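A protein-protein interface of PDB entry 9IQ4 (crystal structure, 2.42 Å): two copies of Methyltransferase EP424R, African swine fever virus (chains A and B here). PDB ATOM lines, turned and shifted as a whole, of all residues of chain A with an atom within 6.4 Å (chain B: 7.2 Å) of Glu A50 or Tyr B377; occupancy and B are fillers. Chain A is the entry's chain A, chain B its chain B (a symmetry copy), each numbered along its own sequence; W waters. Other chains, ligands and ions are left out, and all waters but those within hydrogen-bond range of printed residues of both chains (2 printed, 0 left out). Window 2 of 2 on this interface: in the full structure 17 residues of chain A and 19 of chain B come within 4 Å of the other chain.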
ATOM      1  N   PRO A  46      -6.260  26.349 -23.077  1.00  0.00           N
ATOM      2  CA  PRO A  46      -6.333  26.566 -21.630  1.00  0.00           C
ATOM      3  C   PRO A  46      -7.300  25.594 -20.990  1.00  0.00           C
ATOM      4  O   PRO A  46      -8.227  25.094 -21.624  1.00  0.00           O
ATOM      5  CB  PRO A  46      -6.839  28.006 -21.517  1.00  0.00           C
ATOM      6  CG  PRO A  46      -7.573  28.261 -22.798  1.00  0.00           C
ATOM      7  CD  PRO A  46      -7.134  27.265 -23.831  1.00  0.00           C
ATOM      8  N   SER A  47      -7.075  25.324 -19.710  1.00  0.00           N
ATOM      9  CA  SER A  47      -7.832  24.269 -19.060  1.00  0.00           C
ATOM     10  C   SER A  47      -9.331  24.557 -19.027  1.00  0.00           C
ATOM     11  O   SER A  47     -10.126  23.618 -18.891  1.00  0.00           O
ATOM     12  CB  SER A  47      -7.291  24.056 -17.654  1.00  0.00           C
ATOM     13  OG  SER A  47      -7.415  25.247 -16.905  1.00  0.00           O
ATOM     14  N   ILE A  48      -9.744  25.820 -19.170  1.00  0.00           N
ATOM     15  CA  ILE A  48     -11.178  26.112 -19.178  1.00  0.00           C
ATOM     16  C   ILE A  48     -11.882  25.527 -20.402  1.00  0.00           C
ATOM     17  O   ILE A  48     -13.098  25.296 -20.357  1.00  0.00           O
ATOM     18  CB  ILE A  48     -11.447  27.624 -19.066  1.00  0.00           C
ATOM     19  CG1 ILE A  48     -12.876  27.856 -18.569  1.00  0.00           C
ATOM     20  CG2 ILE A  48     -11.157  28.375 -20.378  1.00  0.00           C
ATOM     21  CD1 ILE A  48     -13.321  29.309 -18.694  1.00  0.00           C
ATOM     22  N   LEU A  49     -11.151  25.256 -21.487  1.00  0.00           N
ATOM     23  CA  LEU A  49     -11.759  24.587 -22.629  1.00  0.00           C
ATOM     24  C   LEU A  49     -12.319  23.216 -22.262  1.00  0.00           C
ATOM     25  O   LEU A  49     -13.268  22.741 -22.902  1.00  0.00           O
ATOM     26  CB  LEU A  49     -10.748  24.455 -23.752  1.00  0.00           C
ATOM     27  CG  LEU A  49     -11.021  25.482 -24.837  1.00  0.00           C
ATOM     28  CD1 LEU A  49      -9.889  25.451 -25.830  1.00  0.00           C
ATOM     29  CD2 LEU A  49     -12.341  25.175 -25.525  1.00  0.00           C
ATOM     30  N   GLU A  50     -11.736  22.560 -21.252  1.00  0.00           N
ATOM     31  CA  GLU A  50     -12.254  21.278 -20.790  1.00  0.00           C
ATOM     32  C   GLU A  50     -13.653  21.425 -20.208  1.00  0.00           C
ATOM     33  O   GLU A  50     -14.523  20.574 -20.417  1.00  0.00           O
ATOM     34  CB  GLU A  50     -11.296  20.685 -19.754  1.00  0.00           C
ATOM     35  CG  GLU A  50     -10.336  19.631 -20.299  1.00  0.00           C
ATOM     36  CD  GLU A  50     -10.946  18.812 -21.442  1.00  0.00           C
ATOM     37  OE1 GLU A  50     -11.816  17.934 -21.177  1.00  0.00           O
ATOM     38  OE2 GLU A  50     -10.554  19.060 -22.611  1.00  0.00           O
ATOM     39  N   LYS A  51     -13.880  22.492 -19.459  1.00  0.00           N
ATOM     40  CA  LYS A  51     -15.202  22.766 -18.916  1.00  0.00           C
ATOM     41  C   LYS A  51     -16.208  23.087 -20.021  1.00  0.00           C
ATOM     42  O   LYS A  51     -17.405  22.791 -19.883  1.00  0.00           O
ATOM     43  CB  LYS A  51     -15.087  23.909 -17.912  1.00  0.00           C
ATOM     44  CG  LYS A  51     -16.255  24.074 -16.986  1.00  0.00           C
ATOM     45  CD  LYS A  51     -15.795  24.606 -15.649  1.00  0.00           C
ATOM     46  CE  LYS A  51     -15.771  26.120 -15.632  1.00  0.00           C
ATOM     47  NZ  LYS A  51     -14.670  26.583 -14.758  1.00  0.00           N
ATOM     48  N   PHE A  52     -15.745  23.670 -21.126  1.00  0.00           N
ATOM     49  CA  PHE A  52     -16.611  23.847 -22.286  1.00  0.00           C
ATOM     50  C   PHE A  52     -16.883  22.516 -22.977  1.00  0.00           C
ATOM     51  O   PHE A  52     -17.988  22.289 -23.495  1.00  0.00           O
ATOM     52  CB  PHE A  52     -15.974  24.819 -23.271  1.00  0.00           C
ATOM     53  CG  PHE A  52     -16.145  26.264 -22.913  1.00  0.00           C
ATOM     54  CD1 PHE A  52     -17.341  26.928 -23.182  1.00  0.00           C
ATOM     55  CD2 PHE A  52     -15.099  26.978 -22.356  1.00  0.00           C
ATOM     56  CE1 PHE A  52     -17.491  28.273 -22.892  1.00  0.00           C
ATOM     57  CE2 PHE A  52     -15.241  28.339 -22.074  1.00  0.00           C
ATOM     58  CZ  PHE A  52     -16.440  28.978 -22.338  1.00  0.00           C
ATOM     59  N   LYS A  53     -15.874  21.641 -23.031  1.00  0.00           N
ATOM     60  CA  LYS A  53     -16.083  20.285 -23.530  1.00  0.00           C
ATOM     61  C   LYS A  53     -17.128  19.548 -22.696  1.00  0.00           C
ATOM     62  O   LYS A  53     -18.009  18.873 -23.239  1.00  0.00           O
ATOM     63  CB  LYS A  53     -14.759  19.524 -23.526  1.00  0.00           C
ATOM     64  CG  LYS A  53     -14.588  18.619 -24.717  1.00  0.00           C
ATOM     65  CD  LYS A  53     -15.217  17.261 -24.454  1.00  0.00           C
ATOM     66  CE  LYS A  53     -15.456  16.484 -25.742  1.00  0.00           C
ATOM     67  NZ  LYS A  53     -16.576  17.085 -26.515  1.00  0.00           N
ATOM     68  N   ARG A  54     -17.063  19.704 -21.371  1.00  0.00           N
ATOM     69  CA  ARG A  54     -18.015  19.051 -20.477  1.00  0.00           C
ATOM     70  C   ARG A  54     -19.420  19.590 -20.687  1.00  0.00           C
ATOM     71  O   ARG A  54     -20.399  18.836 -20.610  1.00  0.00           O
ATOM     72  CB  ARG A  54     -17.595  19.258 -19.021  1.00  0.00           C
ATOM     73  CG  ARG A  54     -16.875  18.096 -18.361  1.00  0.00           C
ATOM     74  CD  ARG A  54     -16.313  18.529 -17.002  1.00  0.00           C
ATOM     75  NE  ARG A  54     -14.897  18.868 -17.111  1.00  0.00           N
ATOM     76  CZ  ARG A  54     -14.303  19.881 -16.499  1.00  0.00           C
ATOM     77  NH1 ARG A  54     -14.976  20.709 -15.710  1.00  0.00           N
ATOM     78  NH2 ARG A  54     -13.000  20.071 -16.684  1.00  0.00           N
ATOM     79  N   ALA A  55     -19.540  20.905 -20.930  1.00  0.00           N
ATOM     80  CA  ALA A  55     -20.845  21.488 -21.202  1.00  0.00           C
ATOM     81  C   ALA A  55     -21.415  20.953 -22.510  1.00  0.00           C
ATOM     82  O   ALA A  55     -22.618  20.663 -22.602  1.00  0.00           O
ATOM     83  CB  ALA A  55     -20.744  23.016 -21.212  1.00  0.00           C
ATOM     84  N   ILE A  57     -20.663  17.958 -23.899  1.00  0.00           N
ATOM     85  CA  ILE A  57     -21.043  16.567 -23.663  1.00  0.00           C
ATOM     86  C   ILE A  57     -22.374  16.498 -22.930  1.00  0.00           C
ATOM     87  O   ILE A  57     -23.243  15.681 -23.256  1.00  0.00           O
ATOM     88  CB  ILE A  57     -19.952  15.826 -22.863  1.00  0.00           C
ATOM     89  CG1 ILE A  57     -18.647  15.702 -23.627  1.00  0.00           C
ATOM     90  CG2 ILE A  57     -20.431  14.414 -22.490  1.00  0.00           C
ATOM     91  CD1 ILE A  57     -17.548  15.201 -22.756  1.00  0.00           C
ATOM     92  N   LEU B  69     -21.961   9.646 -27.393  1.00  0.00           N
ATOM     93  CA  LEU B  69     -20.727   8.912 -27.144  1.00  0.00           C
ATOM     94  C   LEU B  69     -20.619   7.663 -28.006  1.00  0.00           C
ATOM     95  O   LEU B  69     -19.504   7.204 -28.291  1.00  0.00           O
ATOM     96  CB  LEU B  69     -20.642   8.547 -25.665  1.00  0.00           C
ATOM     97  CG  LEU B  69     -20.635   9.712 -24.674  1.00  0.00           C
ATOM     98  CD1 LEU B  69     -20.268   9.185 -23.313  1.00  0.00           C
ATOM     99  CD2 LEU B  69     -19.673  10.825 -25.113  1.00  0.00           C
ATOM    100  N   THR B  75     -14.871   7.345 -28.407  1.00  0.00           N
ATOM    101  CA  THR B  75     -15.617   7.719 -27.214  1.00  0.00           C
ATOM    102  C   THR B  75     -16.424   6.556 -26.671  1.00  0.00           C
ATOM    103  O   THR B  75     -16.613   6.460 -25.454  1.00  0.00           O
ATOM    104  CB  THR B  75     -16.537   8.894 -27.516  1.00  0.00           C
ATOM    105  OG1 THR B  75     -17.419   8.536 -28.589  1.00  0.00           O
ATOM    106  CG2 THR B  75     -15.711  10.131 -27.878  1.00  0.00           C
ATOM    107  N   LYS B  78     -14.078   4.716 -24.456  1.00  0.00           N
ATOM    108  CA  LYS B  78     -13.890   5.433 -23.204  1.00  0.00           C
ATOM    109  C   LYS B  78     -15.150   5.414 -22.347  1.00  0.00           C
ATOM    110  O   LYS B  78     -15.062   5.436 -21.115  1.00  0.00           O
ATOM    111  CB  LYS B  78     -13.430   6.861 -23.503  1.00  0.00           C
ATOM    112  CG  LYS B  78     -12.119   6.864 -24.283  1.00  0.00           C
ATOM    113  CD  LYS B  78     -11.309   8.164 -24.191  1.00  0.00           C
ATOM    114  CE  LYS B  78     -10.166   8.017 -23.166  1.00  0.00           C
ATOM    115  NZ  LYS B  78      -9.592   6.620 -23.047  1.00  0.00           N
ATOM    116  N   LEU B  79     -16.326   5.365 -22.965  1.00  0.00           N
ATOM    117  CA  LEU B  79     -17.538   5.228 -22.168  1.00  0.00           C
ATOM    118  C   LEU B  79     -17.545   3.904 -21.420  1.00  0.00           C
ATOM    119  O   LEU B  79     -17.908   3.845 -20.241  1.00  0.00           O
ATOM    120  CB  LEU B  79     -18.788   5.332 -23.039  1.00  0.00           C
ATOM    121  CG  LEU B  79     -20.039   4.943 -22.251  1.00  0.00           C
ATOM    122  CD1 LEU B  79     -20.341   6.020 -21.216  1.00  0.00           C
ATOM    123  CD2 LEU B  79     -21.215   4.715 -23.146  1.00  0.00           C
ATOM    124  N   GLN B  81     -14.921   2.065 -20.662  1.00  0.00           N
ATOM    125  CA  GLN B  81     -13.899   2.141 -19.628  1.00  0.00           C
ATOM    126  C   GLN B  81     -14.459   2.813 -18.381  1.00  0.00           C
ATOM    127  O   GLN B  81     -14.269   2.332 -17.254  1.00  0.00           O
ATOM    128  CB  GLN B  81     -12.679   2.902 -20.129  1.00  0.00           C
ATOM    129  CG  GLN B  81     -11.944   2.301 -21.303  1.00  0.00           C
ATOM    130  CD  GLN B  81     -10.607   2.990 -21.506  1.00  0.00           C
ATOM    131  OE1 GLN B  81     -10.521   4.041 -22.151  1.00  0.00           O
ATOM    132  NE2 GLN B  81      -9.561   2.423 -20.925  1.00  0.00           N
ATOM    133  N   ILE B  82     -15.160   3.936 -18.566  1.00  0.00           N
ATOM    134  CA  ILE B  82     -15.718   4.652 -17.429  1.00  0.00           C
ATOM    135  C   ILE B  82     -16.731   3.780 -16.706  1.00  0.00           C
ATOM    136  O   ILE B  82     -16.786   3.754 -15.467  1.00  0.00           O
ATOM    137  CB  ILE B  82     -16.348   5.981 -17.887  1.00  0.00           C
ATOM    138  CG1 ILE B  82     -15.265   7.005 -18.229  1.00  0.00           C
ATOM    139  CG2 ILE B  82     -17.280   6.517 -16.816  1.00  0.00           C
ATOM    140  CD1 ILE B  82     -14.882   7.888 -17.085  1.00  0.00           C
ATOM    141  N   LYS B 371     -21.637  11.718 -15.334  1.00  0.00           N
ATOM    142  CA  LYS B 371     -20.780  12.689 -14.681  1.00  0.00           C
ATOM    143  C   LYS B 371     -19.337  12.181 -14.606  1.00  0.00           C
ATOM    144  O   LYS B 371     -18.389  12.960 -14.778  1.00  0.00           O
ATOM    145  CB  LYS B 371     -21.329  13.028 -13.292  1.00  0.00           C
ATOM    146  CG  LYS B 371     -20.980  14.450 -12.845  1.00  0.00           C
ATOM    147  CD  LYS B 371     -21.622  14.828 -11.525  1.00  0.00           C
ATOM    148  CE  LYS B 371     -21.350  16.303 -11.187  1.00  0.00           C
ATOM    149  NZ  LYS B 371     -21.830  17.280 -12.241  1.00  0.00           N
ATOM    150  N   CYS B 372     -19.150  10.876 -14.377  1.00  0.00           N
ATOM    151  CA  CYS B 372     -17.804  10.308 -14.434  1.00  0.00           C
ATOM    152  C   CYS B 372     -17.229  10.418 -15.844  1.00  0.00           C
ATOM    153  O   CYS B 372     -16.087  10.860 -16.024  1.00  0.00           O
ATOM    154  CB  CYS B 372     -17.805   8.845 -13.952  1.00  0.00           C
ATOM    155  SG  CYS B 372     -18.083   8.668 -12.155  1.00  0.00           S
ATOM    156  N   TYR B 373     -18.013  10.044 -16.861  1.00  0.00           N
ATOM    157  CA  TYR B 373     -17.527  10.203 -18.226  1.00  0.00           C
ATOM    158  C   TYR B 373     -17.154  11.649 -18.501  1.00  0.00           C
ATOM    159  O   TYR B 373     -16.085  11.920 -19.035  1.00  0.00           O
ATOM    160  CB  TYR B 373     -18.537   9.723 -19.275  1.00  0.00           C
ATOM    161  CG  TYR B 373     -17.947   9.905 -20.677  1.00  0.00           C
ATOM    162  CD1 TYR B 373     -17.979  11.150 -21.322  1.00  0.00           C
ATOM    163  CD2 TYR B 373     -17.300   8.856 -21.328  1.00  0.00           C
ATOM    164  CE1 TYR B 373     -17.399  11.345 -22.557  1.00  0.00           C
ATOM    165  CE2 TYR B 373     -16.728   9.043 -22.588  1.00  0.00           C
ATOM    166  CZ  TYR B 373     -16.783  10.293 -23.196  1.00  0.00           C
ATOM    167  OH  TYR B 373     -16.222  10.497 -24.431  1.00  0.00           O
ATOM    168  N   ARG B 374     -18.037  12.593 -18.170  1.00  0.00           N
ATOM    169  CA  ARG B 374     -17.775  13.996 -18.503  1.00  0.00           C
ATOM    170  C   ARG B 374     -16.438  14.462 -17.930  1.00  0.00           C
ATOM    171  O   ARG B 374     -15.624  15.057 -18.641  1.00  0.00           O
ATOM    172  CB  ARG B 374     -18.911  14.889 -17.995  1.00  0.00           C
ATOM    173  CG  ARG B 374     -20.180  14.836 -18.850  1.00  0.00           C
ATOM    174  CD  ARG B 374     -21.058  16.065 -18.641  1.00  0.00           C
ATOM    175  NE  ARG B 374     -21.501  16.231 -17.257  1.00  0.00           N
ATOM    176  CZ  ARG B 374     -22.442  15.496 -16.677  1.00  0.00           C
ATOM    177  NH1 ARG B 374     -23.070  14.526 -17.330  1.00  0.00           N
ATOM    178  NH2 ARG B 374     -22.763  15.740 -15.412  1.00  0.00           N
ATOM    179  N   HIS B 375     -16.182  14.164 -16.647  1.00  0.00           N
ATOM    180  CA  HIS B 375     -15.052  14.723 -15.918  1.00  0.00           C
ATOM    181  C   HIS B 375     -13.785  13.897 -16.017  1.00  0.00           C
ATOM    182  O   HIS B 375     -12.711  14.397 -15.662  1.00  0.00           O
ATOM    183  CB  HIS B 375     -15.392  14.857 -14.436  1.00  0.00           C
ATOM    184  CG  HIS B 375     -16.229  16.043 -14.123  1.00  0.00           C
ATOM    185  ND1 HIS B 375     -15.690  17.255 -13.764  1.00  0.00           N
ATOM    186  CD2 HIS B 375     -17.570  16.213 -14.133  1.00  0.00           C
ATOM    187  CE1 HIS B 375     -16.663  18.121 -13.549  1.00  0.00           C
ATOM    188  NE2 HIS B 375     -17.814  17.512 -13.764  1.00  0.00           N
ATOM    189  N   PHE B 376     -13.882  12.639 -16.435  1.00  0.00           N
ATOM    190  CA  PHE B 376     -12.752  11.723 -16.365  1.00  0.00           C
ATOM    191  C   PHE B 376     -12.560  10.918 -17.641  1.00  0.00           C
ATOM    192  O   PHE B 376     -11.715  10.012 -17.644  1.00  0.00           O
ATOM    193  CB  PHE B 376     -12.898  10.742 -15.184  1.00  0.00           C
ATOM    194  CG  PHE B 376     -12.933  11.405 -13.830  1.00  0.00           C
ATOM    195  CD1 PHE B 376     -11.766  11.694 -13.151  1.00  0.00           C
ATOM    196  CD2 PHE B 376     -14.139  11.723 -13.235  1.00  0.00           C
ATOM    197  CE1 PHE B 376     -11.808  12.304 -11.909  1.00  0.00           C
ATOM    198  CE2 PHE B 376     -14.177  12.334 -11.987  1.00  0.00           C
ATOM    199  CZ  PHE B 376     -13.009  12.626 -11.333  1.00  0.00           C
ATOM    200  N   TYR B 377     -13.308  11.214 -18.724  1.00  0.00           N
ATOM    201  CA  TYR B 377     -13.253  10.349 -19.905  1.00  0.00           C
ATOM    202  C   TYR B 377     -11.823  10.181 -20.410  1.00  0.00           C
ATOM    203  O   TYR B 377     -11.464   9.113 -20.909  1.00  0.00           O
ATOM    204  CB  TYR B 377     -14.166  10.865 -21.022  1.00  0.00           C
ATOM    205  CG  TYR B 377     -13.746  12.167 -21.658  1.00  0.00           C
ATOM    206  CD1 TYR B 377     -12.876  12.190 -22.749  1.00  0.00           C
ATOM    207  CD2 TYR B 377     -14.248  13.376 -21.190  1.00  0.00           C
ATOM    208  CE1 TYR B 377     -12.498  13.381 -23.334  1.00  0.00           C
ATOM    209  CE2 TYR B 377     -13.871  14.575 -21.768  1.00  0.00           C
ATOM    210  CZ  TYR B 377     -13.002  14.572 -22.837  1.00  0.00           C
ATOM    211  OH  TYR B 377     -12.644  15.774 -23.400  1.00  0.00           O
ATOM    212  N   ASN B 378     -10.981  11.206 -20.252  1.00  0.00           N
ATOM    213  CA  ASN B 378      -9.559  11.060 -20.541  1.00  0.00           C
ATOM    214  C   ASN B 378      -8.699  10.874 -19.290  1.00  0.00           C
ATOM    215  O   ASN B 378      -7.502  10.606 -19.423  1.00  0.00           O
ATOM    216  CB  ASN B 378      -9.054  12.266 -21.341  1.00  0.00           C
ATOM    217  CG  ASN B 378      -8.406  13.310 -20.466  1.00  0.00           C
ATOM    218  OD1 ASN B 378      -7.187  13.304 -20.261  1.00  0.00           O
ATOM    219  ND2 ASN B 378      -9.220  14.218 -19.930  1.00  0.00           N
ATOM    220  N   LYS B 379      -9.270  10.999 -18.087  1.00  0.00           N
ATOM    221  CA  LYS B 379      -8.533  10.686 -16.864  1.00  0.00           C
ATOM    222  C   LYS B 379      -9.051   9.406 -16.203  1.00  0.00           C
ATOM    223  O   LYS B 379      -9.523   9.433 -15.058  1.00  0.00           O
ATOM    224  CB  LYS B 379      -8.605  11.849 -15.872  1.00  0.00           C
ATOM    225  CG  LYS B 379      -8.889  13.226 -16.460  1.00  0.00           C
ATOM    226  CD  LYS B 379      -8.169  14.298 -15.631  1.00  0.00           C
ATOM    227  CE  LYS B 379      -8.884  15.661 -15.617  1.00  0.00           C
ATOM    228  NZ  LYS B 379      -9.997  15.823 -14.623  1.00  0.00           N
ATOM    229  N   ILE B 380      -8.956   8.273 -16.905  1.00  0.00           N
ATOM    230  CA  ILE B 380      -9.460   7.018 -16.352  1.00  0.00           C
ATOM    231  C   ILE B 380      -8.660   6.614 -15.119  1.00  0.00           C
ATOM    232  O   ILE B 380      -9.233   6.227 -14.084  1.00  0.00           O
ATOM    233  CB  ILE B 380      -9.440   5.908 -17.416  1.00  0.00           C
ATOM    234  CG1 ILE B 380     -10.069   6.403 -18.729  1.00  0.00           C
ATOM    235  CG2 ILE B 380     -10.156   4.656 -16.889  1.00  0.00           C
ATOM    236  CD1 ILE B 380     -11.550   6.139 -18.854  1.00  0.00           C
ATOM    237  N   LEU B 383      -9.744   8.435 -12.161  1.00  0.00           N
ATOM    238  CA  LEU B 383     -11.070   8.090 -11.661  1.00  0.00           C
ATOM    239  C   LEU B 383     -11.005   6.865 -10.761  1.00  0.00           C
ATOM    240  O   LEU B 383     -11.579   6.850  -9.664  1.00  0.00           O
ATOM    241  CB  LEU B 383     -12.017   7.844 -12.830  1.00  0.00           C
ATOM    242  CG  LEU B 383     -13.436   7.460 -12.443  1.00  0.00           C
ATOM    243  CD1 LEU B 383     -14.053   8.506 -11.512  1.00  0.00           C
ATOM    244  CD2 LEU B 383     -14.257   7.275 -13.686  1.00  0.00           C
HETATM  245  O   HOH W   1     -13.175  16.600 -18.545  1.00  0.00           O
HETATM  246  O   HOH W   2     -12.854  18.037 -13.917  1.00  0.00           O
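The side-chain hydroxyl (OH) of Tyr B377 lies within hydrogen-bond range of the side-chain carboxylate (OE1) of Glu A50, at 3.2 Å.
The backbone carbonyl oxygen (O) of His B375 sits at hydrogen-bond distance from the side-chain amino group (NZ) of Lys B379 (3.2 Å).
CD of Lys A53 touches OH of Tyr B377 (3.2 Å). CG of Arg A54 touches O of Arg B374 (3.3 Å). Arg A54 touches His B375 (CD to CE1, 3.5 Å). CD1 of Ile A57 touches CE1 of Tyr B373, at 3.9 Å. Arg B374 touches Ile A57 (CG to CG2, 3.7 Å). CE2 of Tyr B377 touches CD1 of Ile A57 (3.9 Å).
Of the printed residues of chain B, Lys A53 touches Tyr B377 (3.2 Å). Of the printed residues of chain B, Ile A57 touches Tyr B373, Arg B374 and Tyr B377. Of chain A, only Glu A50, Lys A53 and Ile A57 come within 4 Å of Tyr B377. The nearest residue of chain B that does not touch Glu A50 is Asn B378 (4.7 Å). The nearest printed residue of chain A that does not touch Tyr B373 is Lys A53 (6.2 Å).
Of the 11 printed residues of chain A, 4 touch a printed residue of chain B. Hydrophobic or aromatic side chains of chain A that line the printed part of chain B: Ile A57. Along chain A the printed residues that touch a printed residue of chain B span positions 50 to 57. Among the printed residues, 7 pairs touch across the chains. Among the printed residues, no Asp or Glu carboxylate lies within 4 Å of a Lys or Arg side-chain nitrogen of the other chain.
No position is printed for both chains.
Water W1 lies within hydrogen-bond range of the backbone carbonyl oxygen (O) of Arg B374 (2.9 Å), the guanidinium group (NE) of Arg A54 (3.2 Å) and the side-chain carboxylate (OE1) of Glu A50 (3.2 Å). Water W2 lies within hydrogen-bond range of a ring nitrogen (ND1) of His B375 (2.9 Å) and the guanidinium group of Arg A54 (3.4 Å).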
